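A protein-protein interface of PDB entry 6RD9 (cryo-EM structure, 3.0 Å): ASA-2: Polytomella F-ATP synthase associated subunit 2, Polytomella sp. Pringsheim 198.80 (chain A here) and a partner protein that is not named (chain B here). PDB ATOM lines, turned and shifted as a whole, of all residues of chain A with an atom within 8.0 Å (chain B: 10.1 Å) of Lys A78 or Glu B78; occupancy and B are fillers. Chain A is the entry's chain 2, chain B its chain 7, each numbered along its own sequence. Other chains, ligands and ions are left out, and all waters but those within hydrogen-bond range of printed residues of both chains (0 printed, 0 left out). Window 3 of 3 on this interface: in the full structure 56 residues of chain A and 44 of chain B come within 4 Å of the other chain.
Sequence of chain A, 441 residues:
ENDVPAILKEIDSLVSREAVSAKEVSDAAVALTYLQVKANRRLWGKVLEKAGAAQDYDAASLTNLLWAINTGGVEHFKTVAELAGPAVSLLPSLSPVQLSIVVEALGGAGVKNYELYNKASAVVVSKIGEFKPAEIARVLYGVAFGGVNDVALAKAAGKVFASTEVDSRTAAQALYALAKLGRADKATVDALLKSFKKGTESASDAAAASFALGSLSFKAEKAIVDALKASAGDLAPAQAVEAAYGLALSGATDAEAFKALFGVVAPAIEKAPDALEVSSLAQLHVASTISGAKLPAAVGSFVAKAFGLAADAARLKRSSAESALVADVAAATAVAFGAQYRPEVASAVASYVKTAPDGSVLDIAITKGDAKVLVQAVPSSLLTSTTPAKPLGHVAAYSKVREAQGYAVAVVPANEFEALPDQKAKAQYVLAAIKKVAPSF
Printed residues of chain A that touch a printed residue of chain B: Arg A41, Leu A48, Glu A75, His A76 and Lys A78. Hydrophobic or aromatic side chains of chain A that line the printed part of chain B: Leu A48 and His A76. Printed residues of chain B that touch a printed residue of chain A: Leu B15, Ile B74, Ser B75, Leu B76 and Glu B78. Among the printed residues, 10 pairs touch across the chains. Among the printed residues, no Asp or Glu carboxylate lies within 4 Å of a Lys or Arg side-chain nitrogen of the other chain.
O of Ile B74 lies within hydrogen-bond range of NH2 of Arg A41, 2.5 Å away. NH1 of Arg A41 is in hydrogen-bond range of O of Ser B75 (3.0 Å). The backbone carbonyl oxygen (O) of Glu A75 sits at hydrogen-bond distance from the backbone NH (N) of Leu B76 (3.0 Å). NE2 of His A76 sits at hydrogen-bond distance from OE2 of Glu B78. N of Leu B15 lies close to OE1 of Glu A75.
OG1 of Thr A79 is in hydrogen-bond range of ND1 of His A76 (2.4 Å). The side-chain amino group (NZ) of Lys A78 lies within salt-bridge range of the side-chain carboxylate (OE2) of Glu A82 (3.2 Å).
Of the printed residues of chain B, Lys A78 touches Glu B78. Of the printed residues of chain A, Glu B78 touches His A76 and Lys A78. No residue of chain B comes within 4 Å of Phe A77. No residue of chain B comes within 4 Å of Ala A81. No residue of chain A comes within 4 Å of Ala B77. Of the printed residues of chain A, Ile B74 touches Arg A41. Of the printed residues of chain B, Leu A48 touches Leu B76. Printed residues of chain A within 4 Å of Leu B76: Arg A41, Leu A48, Glu A75 and His A76. Of the printed residues of chain A, Ser B75 touches Arg A41 (3.0 Å) and Glu A75 (3.4 Å). Ala A51 touches none of the printed residues of chain B.
Arg A41 touches Leu B76 (O to CD2, 3.4 Å). CD1 of Leu B76 touches CD1 of Leu A48, 3.7 Å away. Glu A75 touches Ser B75 (O to CA, 3.4 Å). CD2 of His A76 touches O of Leu B76 (3.6 Å). Lys A78 touches Glu B78.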
ATOM      1  N   ARG A  41      -2.856  26.068 -13.790  1.00  0.00           N
ATOM      2  CA  ARG A  41      -2.650  24.638 -13.670  1.00  0.00           C
ATOM      3  C   ARG A  41      -2.471  24.212 -12.233  1.00  0.00           C
ATOM      4  O   ARG A  41      -2.831  23.088 -11.882  1.00  0.00           O
ATOM      5  CB  ARG A  41      -1.428  24.210 -14.463  1.00  0.00           C
ATOM      6  CG  ARG A  41      -1.442  24.634 -15.883  1.00  0.00           C
ATOM      7  CD  ARG A  41      -0.087  24.400 -16.478  1.00  0.00           C
ATOM      8  NE  ARG A  41       0.406  23.071 -16.171  1.00  0.00           N
ATOM      9  CZ  ARG A  41       0.151  22.007 -16.914  1.00  0.00           C
ATOM     10  NH1 ARG A  41       0.636  20.825 -16.575  1.00  0.00           N
ATOM     11  NH2 ARG A  41      -0.587  22.129 -18.003  1.00  0.00           N
ATOM     12  N   LEU A  48      -7.099  18.074  -7.728  1.00  0.00           N
ATOM     13  CA  LEU A  48      -6.894  16.648  -7.890  1.00  0.00           C
ATOM     14  C   LEU A  48      -6.003  16.072  -6.808  1.00  0.00           C
ATOM     15  O   LEU A  48      -5.983  14.857  -6.628  1.00  0.00           O
ATOM     16  CB  LEU A  48      -6.320  16.344  -9.267  1.00  0.00           C
ATOM     17  CG  LEU A  48      -7.245  16.601 -10.449  1.00  0.00           C
ATOM     18  CD1 LEU A  48      -6.638  16.060 -11.693  1.00  0.00           C
ATOM     19  CD2 LEU A  48      -8.594  15.981 -10.234  1.00  0.00           C
ATOM     20  N   GLU A  49      -5.265  16.901  -6.084  1.00  0.00           N
ATOM     21  CA  GLU A  49      -4.552  16.407  -4.917  1.00  0.00           C
ATOM     22  C   GLU A  49      -5.510  16.054  -3.798  1.00  0.00           C
ATOM     23  O   GLU A  49      -5.314  15.060  -3.100  1.00  0.00           O
ATOM     24  CB  GLU A  49      -3.561  17.443  -4.435  1.00  0.00           C
ATOM     25  CG  GLU A  49      -2.226  17.302  -5.050  1.00  0.00           C
ATOM     26  CD  GLU A  49      -1.221  18.167  -4.370  1.00  0.00           C
ATOM     27  OE1 GLU A  49      -1.519  19.356  -4.151  1.00  0.00           O
ATOM     28  OE2 GLU A  49      -0.135  17.655  -4.039  1.00  0.00           O
ATOM     29  N   ALA A  51      -8.621  15.316  -4.412  1.00  0.00           N
ATOM     30  CA  ALA A  51      -9.528  14.320  -4.949  1.00  0.00           C
ATOM     31  C   ALA A  51      -9.011  12.914  -4.745  1.00  0.00           C
ATOM     32  O   ALA A  51      -9.794  11.968  -4.798  1.00  0.00           O
ATOM     33  CB  ALA A  51      -9.768  14.572  -6.425  1.00  0.00           C
ATOM     34  N   GLY A  52      -7.719  12.748  -4.537  1.00  0.00           N
ATOM     35  CA  GLY A  52      -7.207  11.452  -4.173  1.00  0.00           C
ATOM     36  C   GLY A  52      -7.272  11.257  -2.678  1.00  0.00           C
ATOM     37  O   GLY A  52      -7.461  10.140  -2.195  1.00  0.00           O
ATOM     38  N   ALA A  53      -7.130  12.348  -1.933  1.00  0.00           N
ATOM     39  CA  ALA A  53      -7.184  12.281  -0.485  1.00  0.00           C
ATOM     40  C   ALA A  53      -8.584  12.066   0.047  1.00  0.00           C
ATOM     41  O   ALA A  53      -8.728  11.572   1.164  1.00  0.00           O
ATOM     42  CB  ALA A  53      -6.622  13.560   0.117  1.00  0.00           C
ATOM     43  N   GLU A  75      -6.061  16.029 -17.201  1.00  0.00           N
ATOM     44  CA  GLU A  75      -5.747  14.622 -17.055  1.00  0.00           C
ATOM     45  C   GLU A  75      -4.626  14.455 -16.054  1.00  0.00           C
ATOM     46  O   GLU A  75      -3.627  15.174 -16.096  1.00  0.00           O
ATOM     47  CB  GLU A  75      -5.391  13.982 -18.391  1.00  0.00           C
ATOM     48  CG  GLU A  75      -4.412  14.748 -19.201  1.00  0.00           C
ATOM     49  CD  GLU A  75      -4.064  14.067 -20.489  1.00  0.00           C
ATOM     50  OE1 GLU A  75      -4.603  12.975 -20.741  1.00  0.00           O
ATOM     51  OE2 GLU A  75      -3.253  14.619 -21.258  1.00  0.00           O
ATOM     52  N   HIS A  76      -4.834  13.543 -15.122  1.00  0.00           N
ATOM     53  CA  HIS A  76      -3.778  13.048 -14.262  1.00  0.00           C
ATOM     54  C   HIS A  76      -4.153  11.603 -14.029  1.00  0.00           C
ATOM     55  O   HIS A  76      -5.176  11.351 -13.402  1.00  0.00           O
ATOM     56  CB  HIS A  76      -3.698  13.820 -12.958  1.00  0.00           C
ATOM     57  CG  HIS A  76      -2.605  13.354 -12.056  1.00  0.00           C
ATOM     58  ND1 HIS A  76      -2.844  12.851 -10.801  1.00  0.00           N
ATOM     59  CD2 HIS A  76      -1.269  13.297 -12.237  1.00  0.00           C
ATOM     60  CE1 HIS A  76      -1.700  12.509 -10.242  1.00  0.00           C
ATOM     61  NE2 HIS A  76      -0.730  12.767 -11.095  1.00  0.00           N
ATOM     62  N   PHE A  77      -3.353  10.672 -14.549  1.00  0.00           N
ATOM     63  CA  PHE A  77      -3.773   9.281 -14.558  1.00  0.00           C
ATOM     64  C   PHE A  77      -3.850   8.693 -13.171  1.00  0.00           C
ATOM     65  O   PHE A  77      -4.719   7.866 -12.921  1.00  0.00           O
ATOM     66  CB  PHE A  77      -2.836   8.427 -15.395  1.00  0.00           C
ATOM     67  CG  PHE A  77      -3.297   7.015 -15.541  1.00  0.00           C
ATOM     68  CD1 PHE A  77      -4.342   6.706 -16.370  1.00  0.00           C
ATOM     69  CD2 PHE A  77      -2.700   6.005 -14.836  1.00  0.00           C
ATOM     70  CE1 PHE A  77      -4.768   5.420 -16.487  1.00  0.00           C
ATOM     71  CE2 PHE A  77      -3.128   4.719 -14.957  1.00  0.00           C
ATOM     72  CZ  PHE A  77      -4.158   4.429 -15.778  1.00  0.00           C
ATOM     73  N   LYS A  78      -2.981   9.110 -12.261  1.00  0.00           N
ATOM     74  CA  LYS A  78      -2.974   8.518 -10.933  1.00  0.00           C
ATOM     75  C   LYS A  78      -4.219   8.891 -10.155  1.00  0.00           C
ATOM     76  O   LYS A  78      -4.777   8.065  -9.437  1.00  0.00           O
ATOM     77  CB  LYS A  78      -1.732   8.958 -10.185  1.00  0.00           C
ATOM     78  CG  LYS A  78      -1.625   8.380  -8.816  1.00  0.00           C
ATOM     79  CD  LYS A  78      -0.565   9.049  -8.034  1.00  0.00           C
ATOM     80  CE  LYS A  78      -0.613   8.565  -6.624  1.00  0.00           C
ATOM     81  NZ  LYS A  78      -2.022   8.474  -6.185  1.00  0.00           N
ATOM     82  N   THR A  79      -4.694  10.114 -10.322  1.00  0.00           N
ATOM     83  CA  THR A  79      -5.857  10.563  -9.575  1.00  0.00           C
ATOM     84  C   THR A  79      -7.135   9.967 -10.118  1.00  0.00           C
ATOM     85  O   THR A  79      -7.979   9.504  -9.350  1.00  0.00           O
ATOM     86  CB  THR A  79      -5.944  12.071  -9.621  1.00  0.00           C
ATOM     87  OG1 THR A  79      -4.688  12.620  -9.219  1.00  0.00           O
ATOM     88  CG2 THR A  79      -7.015  12.536  -8.701  1.00  0.00           C
ATOM     89  N   VAL A  80      -7.282   9.952 -11.437  1.00  0.00           N
ATOM     90  CA  VAL A  80      -8.515   9.490 -12.048  1.00  0.00           C
ATOM     91  C   VAL A  80      -8.633   7.979 -11.944  1.00  0.00           C
ATOM     92  O   VAL A  80      -9.719   7.451 -11.706  1.00  0.00           O
ATOM     93  CB  VAL A  80      -8.577   9.983 -13.497  1.00  0.00           C
ATOM     94  CG1 VAL A  80      -9.842   9.571 -14.152  1.00  0.00           C
ATOM     95  CG2 VAL A  80      -8.473  11.461 -13.508  1.00  0.00           C
ATOM     96  N   ALA A  81      -7.526   7.254 -12.076  1.00  0.00           N
ATOM     97  CA  ALA A  81      -7.622   5.804 -12.036  1.00  0.00           C
ATOM     98  C   ALA A  81      -7.865   5.262 -10.651  1.00  0.00           C
ATOM     99  O   ALA A  81      -8.302   4.121 -10.523  1.00  0.00           O
ATOM    100  CB  ALA A  81      -6.377   5.152 -12.598  1.00  0.00           C
ATOM    101  N   GLU A  82      -7.597   6.040  -9.619  1.00  0.00           N
ATOM    102  CA  GLU A  82      -7.933   5.648  -8.268  1.00  0.00           C
ATOM    103  C   GLU A  82      -9.315   6.112  -7.869  1.00  0.00           C
ATOM    104  O   GLU A  82      -9.784   5.749  -6.791  1.00  0.00           O
ATOM    105  CB  GLU A  82      -6.898   6.193  -7.304  1.00  0.00           C
ATOM    106  CG  GLU A  82      -5.558   5.562  -7.511  1.00  0.00           C
ATOM    107  CD  GLU A  82      -4.580   5.906  -6.437  1.00  0.00           C
ATOM    108  OE1 GLU A  82      -3.607   5.155  -6.266  1.00  0.00           O
ATOM    109  OE2 GLU A  82      -4.780   6.925  -5.752  1.00  0.00           O
ATOM    110  N   LEU A  83      -9.976   6.900  -8.710  1.00  0.00           N
ATOM    111  CA  LEU A  83     -11.394   7.187  -8.570  1.00  0.00           C
ATOM    112  C   LEU A  83     -12.258   6.068  -9.105  1.00  0.00           C
ATOM    113  O   LEU A  83     -13.479   6.161  -9.029  1.00  0.00           O
ATOM    114  CB  LEU A  83     -11.763   8.473  -9.296  1.00  0.00           C
ATOM    115  CG  LEU A  83     -11.262   9.786  -8.732  1.00  0.00           C
ATOM    116  CD1 LEU A  83     -11.599  10.895  -9.660  1.00  0.00           C
ATOM    117  CD2 LEU A  83     -11.889  10.009  -7.417  1.00  0.00           C
ATOM    118  N   ALA A  84     -11.658   5.036  -9.674  1.00  0.00           N
ATOM    119  CA  ALA A  84     -12.381   3.838 -10.048  1.00  0.00           C
ATOM    120  C   ALA A  84     -12.598   2.909  -8.875  1.00  0.00           C
ATOM    121  O   ALA A  84     -13.235   1.870  -9.042  1.00  0.00           O
ATOM    122  CB  ALA A  84     -11.633   3.098 -11.146  1.00  0.00           C
ATOM    123  N   VAL A 111      -8.322   4.302 -18.003  1.00  0.00           N
ATOM    124  CA  VAL A 111      -8.183   3.543 -16.772  1.00  0.00           C
ATOM    125  C   VAL A 111      -8.412   2.073 -17.073  1.00  0.00           C
ATOM    126  O   VAL A 111      -9.512   1.669 -17.459  1.00  0.00           O
ATOM    127  CB  VAL A 111      -9.168   4.054 -15.721  1.00  0.00           C
ATOM    128  CG1 VAL A 111      -9.081   3.253 -14.476  1.00  0.00           C
ATOM    129  CG2 VAL A 111      -8.905   5.489 -15.464  1.00  0.00           C
ATOM    130  N   LEU B  15      -6.308  11.492 -21.460  1.00  0.00           N
ATOM    131  CA  LEU B  15      -7.542  11.831 -22.136  1.00  0.00           C
ATOM    132  C   LEU B  15      -7.403  11.648 -23.626  1.00  0.00           C
ATOM    133  O   LEU B  15      -6.307  11.714 -24.163  1.00  0.00           O
ATOM    134  CB  LEU B  15      -7.950  13.259 -21.818  1.00  0.00           C
ATOM    135  CG  LEU B  15      -9.094  13.394 -20.835  1.00  0.00           C
ATOM    136  CD1 LEU B  15      -9.409  14.834 -20.672  1.00  0.00           C
ATOM    137  CD2 LEU B  15     -10.293  12.673 -21.378  1.00  0.00           C
ATOM    138  N   ILE B  74      -4.791  19.808 -19.903  1.00  0.00           N
ATOM    139  CA  ILE B  74      -3.947  20.350 -18.842  1.00  0.00           C
ATOM    140  C   ILE B  74      -2.721  19.475 -18.639  1.00  0.00           C
ATOM    141  O   ILE B  74      -1.587  19.960 -18.713  1.00  0.00           O
ATOM    142  CB  ILE B  74      -4.736  20.511 -17.534  1.00  0.00           C
ATOM    143  CG1 ILE B  74      -5.776  21.608 -17.670  1.00  0.00           C
ATOM    144  CG2 ILE B  74      -3.800  20.893 -16.427  1.00  0.00           C
ATOM    145  CD1 ILE B  74      -5.179  22.967 -17.831  1.00  0.00           C
ATOM    146  N   SER B  75      -2.943  18.184 -18.380  1.00  0.00           N
ATOM    147  CA  SER B  75      -1.911  17.164 -18.186  1.00  0.00           C
ATOM    148  C   SER B  75      -0.992  17.518 -17.016  1.00  0.00           C
ATOM    149  O   SER B  75       0.162  17.907 -17.174  1.00  0.00           O
ATOM    150  CB  SER B  75      -1.119  16.903 -19.466  1.00  0.00           C
ATOM    151  OG  SER B  75      -0.214  15.842 -19.256  1.00  0.00           O
ATOM    152  N   LEU B  76      -1.586  17.417 -15.834  1.00  0.00           N
ATOM    153  CA  LEU B  76      -0.895  17.677 -14.585  1.00  0.00           C
ATOM    154  C   LEU B  76       0.200  16.658 -14.351  1.00  0.00           C
ATOM    155  O   LEU B  76       0.100  15.501 -14.755  1.00  0.00           O
ATOM    156  CB  LEU B  76      -1.879  17.628 -13.435  1.00  0.00           C
ATOM    157  CG  LEU B  76      -2.933  18.699 -13.491  1.00  0.00           C
ATOM    158  CD1 LEU B  76      -3.906  18.374 -12.458  1.00  0.00           C
ATOM    159  CD2 LEU B  76      -2.268  19.983 -13.194  1.00  0.00           C
ATOM    160  N   ALA B  77       1.258  17.098 -13.687  1.00  0.00           N
ATOM    161  CA  ALA B  77       2.364  16.212 -13.399  1.00  0.00           C
ATOM    162  C   ALA B  77       3.044  16.682 -12.139  1.00  0.00           C
ATOM    163  O   ALA B  77       3.104  17.876 -11.859  1.00  0.00           O
ATOM    164  CB  ALA B  77       3.366  16.164 -14.538  1.00  0.00           C
ATOM    165  N   GLU B  78       3.578  15.729 -11.399  1.00  0.00           N
ATOM    166  CA  GLU B  78       4.007  15.962 -10.040  1.00  0.00           C
ATOM    167  C   GLU B  78       5.433  16.469 -10.024  1.00  0.00           C
ATOM    168  O   GLU B  78       6.306  15.905 -10.682  1.00  0.00           O
ATOM    169  CB  GLU B  78       3.886  14.679  -9.237  1.00  0.00           C
ATOM    170  CG  GLU B  78       2.520  14.094  -9.353  1.00  0.00           C
ATOM    171  CD  GLU B  78       2.282  12.983  -8.392  1.00  0.00           C
ATOM    172  OE1 GLU B  78       3.209  12.651  -7.647  1.00  0.00           O
ATOM    173  OE2 GLU B  78       1.170  12.433  -8.371  1.00  0.00           O
ATOM    174  N   VAL B  79       5.658  17.537  -9.277  1.00  0.00           N
ATOM    175  CA  VAL B  79       6.993  18.063  -9.057  1.00  0.00           C
ATOM    176  C   VAL B  79       7.503  17.441  -7.771  1.00  0.00           C
ATOM    177  O   VAL B  79       7.045  17.782  -6.683  1.00  0.00           O
ATOM    178  CB  VAL B  79       6.982  19.588  -8.973  1.00  0.00           C
ATOM    179  CG1 VAL B  79       8.339  20.082  -8.610  1.00  0.00           C
ATOM    180  CG2 VAL B  79       6.556  20.146 -10.280  1.00  0.00           C
ATOM    181  N   ALA B  80       8.438  16.519  -7.891  1.00  0.00           N
ATOM    182  CA  ALA B  80       8.928  15.778  -6.750  1.00  0.00           C
ATOM    183  C   ALA B  80      10.336  16.224  -6.424  1.00  0.00           C
ATOM    184  O   ALA B  80      11.031  16.793  -7.262  1.00  0.00           O
ATOM    185  CB  ALA B  80       8.896  14.286  -7.029  1.00  0.00           C
ATOM    186  N   ARG B  81      10.740  15.992  -5.181  1.00  0.00           N
ATOM    187  CA  ARG B  81      12.083  16.377  -4.782  1.00  0.00           C
ATOM    188  C   ARG B  81      13.106  15.503  -5.463  1.00  0.00           C
ATOM    189  O   ARG B  81      14.078  15.998  -6.033  1.00  0.00           O
ATOM    190  CB  ARG B  81      12.244  16.291  -3.277  1.00  0.00           C
ATOM    191  CG  ARG B  81      13.646  16.533  -2.847  1.00  0.00           C
ATOM    192  CD  ARG B  81      13.724  16.832  -1.410  1.00  0.00           C
ATOM    193  NE  ARG B  81      15.100  16.978  -0.975  1.00  0.00           N
ATOM    194  CZ  ARG B  81      15.784  16.013  -0.389  1.00  0.00           C
ATOM    195  NH1 ARG B  81      17.028  16.213  -0.010  1.00  0.00           N
ATOM    196  NH2 ARG B  81      15.214  14.843  -0.186  1.00  0.00           N
ATOM    197  N   ILE B  82      12.888  14.200  -5.442  1.00  0.00           N
ATOM    198  CA  ILE B  82      13.736  13.249  -6.134  1.00  0.00           C
ATOM    199  C   ILE B  82      12.975  12.555  -7.251  1.00  0.00           C
ATOM    200  O   ILE B  82      13.287  12.738  -8.422  1.00  0.00           O
ATOM    201  CB  ILE B  82      14.351  12.241  -5.147  1.00  0.00           C
ATOM    202  CG1 ILE B  82      15.289  12.991  -4.223  1.00  0.00           C
ATOM    203  CG2 ILE B  82      15.098  11.193  -5.881  1.00  0.00           C
ATOM    204  CD1 ILE B  82      15.907  12.162  -3.196  1.00  0.00           C
ATOM    205  N   SER B  83      11.933  11.812  -6.914  1.00  0.00           N
ATOM    206  CA  SER B  83      11.080  11.209  -7.922  1.00  0.00           C
ATOM    207  C   SER B  83       9.747  10.912  -7.273  1.00  0.00           C
ATOM    208  O   SER B  83       9.581  11.081  -6.072  1.00  0.00           O
ATOM    209  CB  SER B  83      11.708   9.954  -8.516  1.00  0.00           C
ATOM    210  OG  SER B  83      12.057   9.024  -7.523  1.00  0.00           O
ATOM    211  N   VAL B  84       8.781  10.520  -8.090  1.00  0.00           N
ATOM    212  CA  VAL B  84       7.480  10.146  -7.565  1.00  0.00           C
ATOM    213  C   VAL B  84       7.548   8.799  -6.883  1.00  0.00           C
ATOM    214  O   VAL B  84       6.811   8.543  -5.932  1.00  0.00           O
ATOM    215  CB  VAL B  84       6.454  10.164  -8.700  1.00  0.00           C
ATOM    216  CG1 VAL B  84       5.096  10.008  -8.181  1.00  0.00           C
ATOM    217  CG2 VAL B  84       6.529  11.460  -9.386  1.00  0.00           C
ATOM    218  N   LEU B  85       8.434   7.924  -7.335  1.00  0.00           N
ATOM    219  CA  LEU B  85       8.610   6.637  -6.684  1.00  0.00           C
ATOM    220  C   LEU B  85       9.198   6.806  -5.302  1.00  0.00           C
ATOM    221  O   LEU B  85       8.691   6.245  -4.332  1.00  0.00           O
ATOM    222  CB  LEU B  85       9.512   5.753  -7.521  1.00  0.00           C
ATOM    223  CG  LEU B  85      10.013   4.509  -6.829  1.00  0.00           C
ATOM    224  CD1 LEU B  85       8.900   3.586  -6.694  1.00  0.00           C
ATOM    225  CD2 LEU B  85      11.091   3.890  -7.613  1.00  0.00           C
ATOM    226  N   HIS B  86      10.261   7.591  -5.200  1.00  0.00           N
ATOM    227  CA  HIS B  86      10.956   7.811  -3.947  1.00  0.00           C
ATOM    228  C   HIS B  86      10.082   8.521  -2.942  1.00  0.00           C
ATOM    229  O   HIS B  86      10.112   8.193  -1.762  1.00  0.00           O
ATOM    230  CB  HIS B  86      12.198   8.619  -4.237  1.00  0.00           C
ATOM    231  CG  HIS B  86      13.016   8.937  -3.040  1.00  0.00           C
ATOM    232  ND1 HIS B  86      14.160   8.248  -2.731  1.00  0.00           N
ATOM    233  CD2 HIS B  86      12.895   9.904  -2.107  1.00  0.00           C
ATOM    234  CE1 HIS B  86      14.689   8.758  -1.640  1.00  0.00           C
ATOM    235  NE2 HIS B  86      13.942   9.766  -1.244  1.00  0.00           N
ATOM    236  N   SER B  87       9.282   9.470  -3.390  1.00  0.00           N
ATOM    237  CA  SER B  87       8.399  10.203  -2.507  1.00  0.00           C
ATOM    238  C   SER B  87       7.259   9.361  -1.998  1.00  0.00           C
ATOM    239  O   SER B  87       6.641   9.726  -1.011  1.00  0.00           O
ATOM    240  CB  SER B  87       7.848  11.405  -3.234  1.00  0.00           C
ATOM    241  OG  SER B  87       8.891  12.317  -3.476  1.00  0.00           O
ATOM    242  N   SER B  88       6.945   8.265  -2.664  1.00  0.00           N
ATOM    243  CA  SER B  88       5.896   7.380  -2.201  1.00  0.00           C
ATOM    244  C   SER B  88       6.420   6.361  -1.225  1.00  0.00           C
ATOM    245  O   SER B  88       5.656   5.831  -0.422  1.00  0.00           O
ATOM    246  CB  SER B  88       5.279   6.666  -3.377  1.00  0.00           C
ATOM    247  OG  SER B  88       6.109   5.596  -3.726  1.00  0.00           O
ATOM    248  N   ASN B  91       6.969   8.668   1.872  1.00  0.00           N
ATOM    249  CA  ASN B  91       5.705   8.925   2.530  1.00  0.00           C
ATOM    250  C   ASN B  91       5.245   7.724   3.316  1.00  0.00           C
ATOM    251  O   ASN B  91       4.531   7.872   4.301  1.00  0.00           O
ATOM    252  CB  ASN B  91       4.661   9.313   1.511  1.00  0.00           C
ATOM    253  CG  ASN B  91       3.370   9.660   2.121  1.00  0.00           C
ATOM    254  OD1 ASN B  91       3.270  10.611   2.867  1.00  0.00           O
ATOM    255  ND2 ASN B  91       2.352   8.892   1.810  1.00  0.00           N
